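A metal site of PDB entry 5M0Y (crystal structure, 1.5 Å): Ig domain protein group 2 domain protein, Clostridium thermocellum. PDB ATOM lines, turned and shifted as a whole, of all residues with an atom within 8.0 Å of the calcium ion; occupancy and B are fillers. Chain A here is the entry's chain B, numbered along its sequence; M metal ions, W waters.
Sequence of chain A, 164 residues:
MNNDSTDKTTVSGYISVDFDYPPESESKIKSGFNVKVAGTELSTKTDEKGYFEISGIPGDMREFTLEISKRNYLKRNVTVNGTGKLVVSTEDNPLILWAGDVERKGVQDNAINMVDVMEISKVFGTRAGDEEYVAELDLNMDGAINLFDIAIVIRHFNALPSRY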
ATOM      1  N   ASP A  20       8.664  -9.939  18.334  1.00  0.00           N
ATOM      2  CA  ASP A  20       9.710  -8.985  18.686  1.00  0.00           C
ATOM      3  C   ASP A  20       9.251  -8.060  19.813  1.00  0.00           C
ATOM      4  O   ASP A  20       8.078  -7.705  19.902  1.00  0.00           O
ATOM      5  CB  ASP A  20      10.132  -8.147  17.469  1.00  0.00           C
ATOM      6  CG  ASP A  20      10.921  -8.960  16.447  1.00  0.00           C
ATOM      7  OD1 ASP A  20      11.839  -9.712  16.853  1.00  0.00           O
ATOM      8  OD2 ASP A  20      10.621  -8.836  15.240  1.00  0.00           O
ATOM      9  N   PRO A  22      11.089  -4.893  22.801  1.00  0.00           N
ATOM     10  CA  PRO A  22      12.310  -4.150  23.132  1.00  0.00           C
ATOM     11  C   PRO A  22      13.189  -4.949  24.103  1.00  0.00           C
ATOM     12  O   PRO A  22      12.653  -5.522  25.053  1.00  0.00           O
ATOM     13  CB  PRO A  22      11.773  -2.882  23.824  1.00  0.00           C
ATOM     14  CG  PRO A  22      10.315  -2.829  23.524  1.00  0.00           C
ATOM     15  CD  PRO A  22       9.888  -4.246  23.356  1.00  0.00           C
ATOM     16  N   ILE A 120      -8.285  -5.651  22.485  1.00  0.00           N
ATOM     17  CA  ILE A 120      -7.134  -4.745  22.382  1.00  0.00           C
ATOM     18  C   ILE A 120      -7.573  -3.414  21.790  1.00  0.00           C
ATOM     19  O   ILE A 120      -7.137  -2.351  22.244  1.00  0.00           O
ATOM     20  CB  ILE A 120      -5.983  -5.380  21.567  1.00  0.00           C
ATOM     21  CG1 ILE A 120      -5.434  -6.596  22.311  1.00  0.00           C
ATOM     22  CG2 ILE A 120      -4.851  -4.371  21.338  1.00  0.00           C
ATOM     23  CD1 ILE A 120      -4.553  -7.482  21.477  1.00  0.00           C
ATOM     24  N   THR A 126      -3.388   4.013  23.258  1.00  0.00           N
ATOM     25  CA  THR A 126      -3.014   4.429  24.611  1.00  0.00           C
ATOM     26  C   THR A 126      -1.531   4.185  24.831  1.00  0.00           C
ATOM     27  O   THR A 126      -0.931   3.346  24.143  1.00  0.00           O
ATOM     28  CB  THR A 126      -3.829   3.714  25.713  1.00  0.00           C
ATOM     29  OG1 THR A 126      -3.668   2.303  25.574  1.00  0.00           O
ATOM     30  CG2 THR A 126      -5.313   4.076  25.617  1.00  0.00           C
ATOM     31  N   TYR A 133      -4.674   3.136  29.439  1.00  0.00           N
ATOM     32  CA  TYR A 133      -3.667   2.107  29.111  1.00  0.00           C
ATOM     33  C   TYR A 133      -3.798   0.927  30.080  1.00  0.00           C
ATOM     34  O   TYR A 133      -3.945   1.122  31.278  1.00  0.00           O
ATOM     35  CB  TYR A 133      -2.259   2.705  29.159  1.00  0.00           C
ATOM     36  CG  TYR A 133      -1.104   1.737  29.033  1.00  0.00           C
ATOM     37  CD1 TYR A 133      -0.558   1.414  27.782  1.00  0.00           C
ATOM     38  CD2 TYR A 133      -0.512   1.182  30.164  1.00  0.00           C
ATOM     39  CE1 TYR A 133       0.526   0.552  27.675  1.00  0.00           C
ATOM     40  CE2 TYR A 133       0.570   0.324  30.067  1.00  0.00           C
ATOM     41  CZ  TYR A 133       1.084   0.008  28.827  1.00  0.00           C
ATOM     42  OH  TYR A 133       2.168  -0.834  28.745  1.00  0.00           O
ATOM     43  N   ALA A 135      -1.725  -2.455  30.974  1.00  0.00           N
ATOM     44  CA  ALA A 135      -0.413  -3.092  30.787  1.00  0.00           C
ATOM     45  C   ALA A 135      -0.488  -4.475  30.161  1.00  0.00           C
ATOM     46  O   ALA A 135       0.294  -4.797  29.279  1.00  0.00           O
ATOM     47  CB  ALA A 135       0.329  -3.156  32.109  1.00  0.00           C
ATOM     48  N   LEU A 137      -2.636  -5.711  28.136  1.00  0.00           N
ATOM     49  CA  LEU A 137      -2.993  -5.670  26.716  1.00  0.00           C
ATOM     50  C   LEU A 137      -1.881  -5.101  25.820  1.00  0.00           C
ATOM     51  O   LEU A 137      -1.985  -5.192  24.599  1.00  0.00           O
ATOM     52  CB  LEU A 137      -4.293  -4.881  26.530  1.00  0.00           C
ATOM     53  CG  LEU A 137      -5.523  -5.487  27.208  1.00  0.00           C
ATOM     54  CD1 LEU A 137      -6.719  -4.562  27.059  1.00  0.00           C
ATOM     55  CD2 LEU A 137      -5.841  -6.859  26.630  1.00  0.00           C
ATOM     56  N   ASP A 138      -0.838  -4.527  26.422  1.00  0.00           N
ATOM     57  CA  ASP A 138       0.374  -4.142  25.714  1.00  0.00           C
ATOM     58  C   ASP A 138       1.210  -5.406  25.542  1.00  0.00           C
ATOM     59  O   ASP A 138       2.122  -5.677  26.334  1.00  0.00           O
ATOM     60  CB  ASP A 138       1.119  -3.057  26.521  1.00  0.00           C
ATOM     61  CG  ASP A 138       2.369  -2.547  25.827  1.00  0.00           C
ATOM     62  OD1 ASP A 138       2.689  -2.983  24.704  1.00  0.00           O
ATOM     63  OD2 ASP A 138       3.040  -1.674  26.414  1.00  0.00           O
ATOM     64  N   LEU A 139       0.896  -6.175  24.510  1.00  0.00           N
ATOM     65  CA  LEU A 139       1.413  -7.540  24.379  1.00  0.00           C
ATOM     66  C   LEU A 139       2.937  -7.592  24.212  1.00  0.00           C
ATOM     67  O   LEU A 139       3.572  -8.456  24.811  1.00  0.00           O
ATOM     68  CB  LEU A 139       0.730  -8.284  23.230  1.00  0.00           C
ATOM     69  CG  LEU A 139      -0.785  -8.484  23.355  1.00  0.00           C
ATOM     70  CD1 LEU A 139      -1.286  -9.281  22.152  1.00  0.00           C
ATOM     71  CD2 LEU A 139      -1.176  -9.142  24.660  1.00  0.00           C
ATOM     72  N   ASN A 140       3.509  -6.679  23.432  1.00  0.00           N
ATOM     73  CA  ASN A 140       4.981  -6.599  23.289  1.00  0.00           C
ATOM     74  C   ASN A 140       5.684  -5.749  24.366  1.00  0.00           C
ATOM     75  O   ASN A 140       6.903  -5.590  24.326  1.00  0.00           O
ATOM     76  CB  ASN A 140       5.399  -6.182  21.883  1.00  0.00           C
ATOM     77  CG  ASN A 140       4.887  -4.810  21.494  1.00  0.00           C
ATOM     78  OD1 ASN A 140       4.382  -4.074  22.326  1.00  0.00           O
ATOM     79  ND2 ASN A 140       4.999  -4.487  20.208  1.00  0.00           N
ATOM     80  N   MET A 141       4.888  -5.187  25.283  1.00  0.00           N
ATOM     81  CA  MET A 141       5.379  -4.471  26.467  1.00  0.00           C
ATOM     82  C   MET A 141       6.362  -3.349  26.097  1.00  0.00           C
ATOM     83  O   MET A 141       7.414  -3.183  26.724  1.00  0.00           O
ATOM     84  CB  MET A 141       6.004  -5.451  27.478  1.00  0.00           C
ATOM     85  CG  MET A 141       5.047  -6.550  27.924  1.00  0.00           C
ATOM     86  SD  MET A 141       5.602  -7.460  29.387  1.00  0.00           S
ATOM     87  CE  MET A 141       4.605  -8.934  29.232  1.00  0.00           C
ATOM     88  N   ASP A 142       5.988  -2.567  25.077  1.00  0.00           N
ATOM     89  CA  ASP A 142       6.797  -1.440  24.603  1.00  0.00           C
ATOM     90  C   ASP A 142       6.256  -0.070  25.059  1.00  0.00           C
ATOM     91  O   ASP A 142       6.763   0.966  24.613  1.00  0.00           O
ATOM     92  CB  ASP A 142       6.984  -1.485  23.076  1.00  0.00           C
ATOM     93  CG  ASP A 142       5.698  -1.194  22.295  1.00  0.00           C
ATOM     94  OD1 ASP A 142       4.596  -1.124  22.903  1.00  0.00           O
ATOM     95  OD2 ASP A 142       5.789  -1.067  21.058  1.00  0.00           O
ATOM     96  N   GLY A 143       5.232  -0.072  25.918  1.00  0.00           N
ATOM     97  CA  GLY A 143       4.663   1.160  26.460  1.00  0.00           C
ATOM     98  C   GLY A 143       3.581   1.823  25.622  1.00  0.00           C
ATOM     99  O   GLY A 143       3.157   2.939  25.937  1.00  0.00           O
ATOM    100  N   ALA A 144       3.129   1.154  24.550  1.00  0.00           N
ATOM    101  CA  ALA A 144       2.035   1.660  23.731  1.00  0.00           C
ATOM    102  C   ALA A 144       1.154   0.490  23.301  1.00  0.00           C
ATOM    103  O   ALA A 144       1.664  -0.613  23.093  1.00  0.00           O
ATOM    104  CB  ALA A 144       2.560   2.393  22.514  1.00  0.00           C
ATOM    105  N   ILE A 145      -0.155   0.729  23.186  1.00  0.00           N
ATOM    106  CA  ILE A 145      -1.067  -0.269  22.625  1.00  0.00           C
ATOM    107  C   ILE A 145      -1.471   0.206  21.248  1.00  0.00           C
ATOM    108  O   ILE A 145      -2.133   1.241  21.097  1.00  0.00           O
ATOM    109  CB  ILE A 145      -2.290  -0.494  23.525  1.00  0.00           C
ATOM    110  CG1 ILE A 145      -1.823  -1.040  24.874  1.00  0.00           C
ATOM    111  CG2 ILE A 145      -3.246  -1.488  22.860  1.00  0.00           C
ATOM    112  CD1 ILE A 145      -2.895  -1.129  25.938  1.00  0.00           C
ATOM    113  N   ASN A 146      -1.064  -0.552  20.229  1.00  0.00           N
ATOM    114  CA  ASN A 146      -1.198  -0.103  18.853  1.00  0.00           C
ATOM    115  C   ASN A 146      -1.175  -1.274  17.868  1.00  0.00           C
ATOM    116  O   ASN A 146      -1.411  -2.419  18.276  1.00  0.00           O
ATOM    117  CB  ASN A 146      -0.137   0.979  18.580  1.00  0.00           C
ATOM    118  CG  ASN A 146       1.293   0.462  18.650  1.00  0.00           C
ATOM    119  OD1 ASN A 146       1.559  -0.720  18.466  1.00  0.00           O
ATOM    120  ND2 ASN A 146       2.237   1.373  18.882  1.00  0.00           N
ATOM    121  N   LEU A 147      -0.942  -1.013  16.587  1.00  0.00           N
ATOM    122  CA  LEU A 147      -1.054  -2.055  15.571  1.00  0.00           C
ATOM    123  C   LEU A 147      -0.036  -3.184  15.687  1.00  0.00           C
ATOM    124  O   LEU A 147      -0.316  -4.287  15.235  1.00  0.00           O
ATOM    125  CB  LEU A 147      -1.036  -1.450  14.164  1.00  0.00           C
ATOM    126  CG  LEU A 147      -2.241  -0.565  13.827  1.00  0.00           C
ATOM    127  CD1 LEU A 147      -1.960   0.245  12.566  1.00  0.00           C
ATOM    128  CD2 LEU A 147      -3.522  -1.367  13.707  1.00  0.00           C
ATOM    129  N   PHE A 148       1.125  -2.940  16.314  1.00  0.00           N
ATOM    130  CA  PHE A 148       2.074  -4.033  16.578  1.00  0.00           C
ATOM    131  C   PHE A 148       1.477  -5.086  17.504  1.00  0.00           C
ATOM    132  O   PHE A 148       1.699  -6.274  17.290  1.00  0.00           O
ATOM    133  CB  PHE A 148       3.373  -3.513  17.191  1.00  0.00           C
ATOM    134  CG  PHE A 148       4.256  -2.725  16.253  1.00  0.00           C
ATOM    135  CD1 PHE A 148       4.504  -3.163  14.952  1.00  0.00           C
ATOM    136  CD2 PHE A 148       4.875  -1.563  16.690  1.00  0.00           C
ATOM    137  CE1 PHE A 148       5.339  -2.446  14.106  1.00  0.00           C
ATOM    138  CE2 PHE A 148       5.709  -0.832  15.839  1.00  0.00           C
ATOM    139  CZ  PHE A 148       5.941  -1.280  14.550  1.00  0.00           C
ATOM    140  N   ASP A 149       0.711  -4.649  18.504  1.00  0.00           N
ATOM    141  CA  ASP A 149       0.050  -5.576  19.442  1.00  0.00           C
ATOM    142  C   ASP A 149      -1.054  -6.359  18.736  1.00  0.00           C
ATOM    143  O   ASP A 149      -1.191  -7.570  18.938  1.00  0.00           O
ATOM    144  CB  ASP A 149      -0.510  -4.819  20.641  1.00  0.00           C
ATOM    145  CG  ASP A 149       0.556  -4.049  21.367  1.00  0.00           C
ATOM    146  OD1 ASP A 149       1.418  -4.666  22.023  1.00  0.00           O
ATOM    147  OD2 ASP A 149       0.572  -2.803  21.278  1.00  0.00           O
ATOM    148  N   ILE A 150      -1.838  -5.663  17.910  1.00  0.00           N
ATOM    149  CA  ILE A 150      -2.860  -6.323  17.105  1.00  0.00           C
ATOM    150  C   ILE A 150      -2.241  -7.318  16.110  1.00  0.00           C
ATOM    151  O   ILE A 150      -2.759  -8.428  15.935  1.00  0.00           O
ATOM    152  CB  ILE A 150      -3.798  -5.290  16.425  1.00  0.00           C
ATOM    153  CG1 ILE A 150      -4.690  -4.662  17.503  1.00  0.00           C
ATOM    154  CG2 ILE A 150      -4.647  -5.938  15.335  1.00  0.00           C
ATOM    155  CD1 ILE A 150      -5.461  -3.435  17.054  1.00  0.00           C
ATOM    156  N   ILE A 152       0.440  -9.067  16.475  1.00  0.00           N
ATOM    157  CA  ILE A 152       0.838 -10.256  17.237  1.00  0.00           C
ATOM    158  C   ILE A 152      -0.342 -11.235  17.335  1.00  0.00           C
ATOM    159  O   ILE A 152      -0.184 -12.431  17.121  1.00  0.00           O
ATOM    160  CB  ILE A 152       1.388  -9.903  18.643  1.00  0.00           C
ATOM    161  CG1 ILE A 152       2.761  -9.244  18.514  1.00  0.00           C
ATOM    162  CG2 ILE A 152       1.485 -11.130  19.544  1.00  0.00           C
ATOM    163  CD1 ILE A 152       3.225  -8.490  19.741  1.00  0.00           C
HETATM  164 CA    CA M   1       2.672  -2.522  22.431  1.00  0.00          CA
HETATM  165  O   HOH W   1       3.371  -1.870  20.229  1.00  0.00           O
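The side-chain carboxylate of Asp 149 lies close to the backbone NH of Asn 146, 3.0 Å away. The side-chain carboxylate of Asp 138 sits at hydrogen-bond distance from the side-chain hydroxyl of Tyr 133, 2.6 Å away. N of Leu 139 lies close to OD1 of Asp 149 (3.0 Å). The side-chain carboxylate (OD2) of Asp 138 sits at hydrogen-bond distance from the backbone NH (N) of Gly 143 (2.8 Å). The backbone NH (N) of Met 141 lies close to the side-chain carboxylate (OD1) of Asp 138, 3.2 Å away.
The nearest printed residue that does not touch the calcium ion is Ile 145 (4.4 Å).
The calcium ion is bound by O of Ala 144 (2.3 Å), OD1 of Asn 140 (2.3 Å), OD1 of Asp 138 (2.3 Å), water W1 (2.4 Å), OD2 of Asp 149 (2.4 Å), OD1 of Asp 142 (2.4 Å) and OD1 of Asp 149 (2.5 Å).
Water W1 lies within hydrogen-bond range of OD2 of Asp 142, OD1 of Asn 146 and ND2 of Asn 140.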
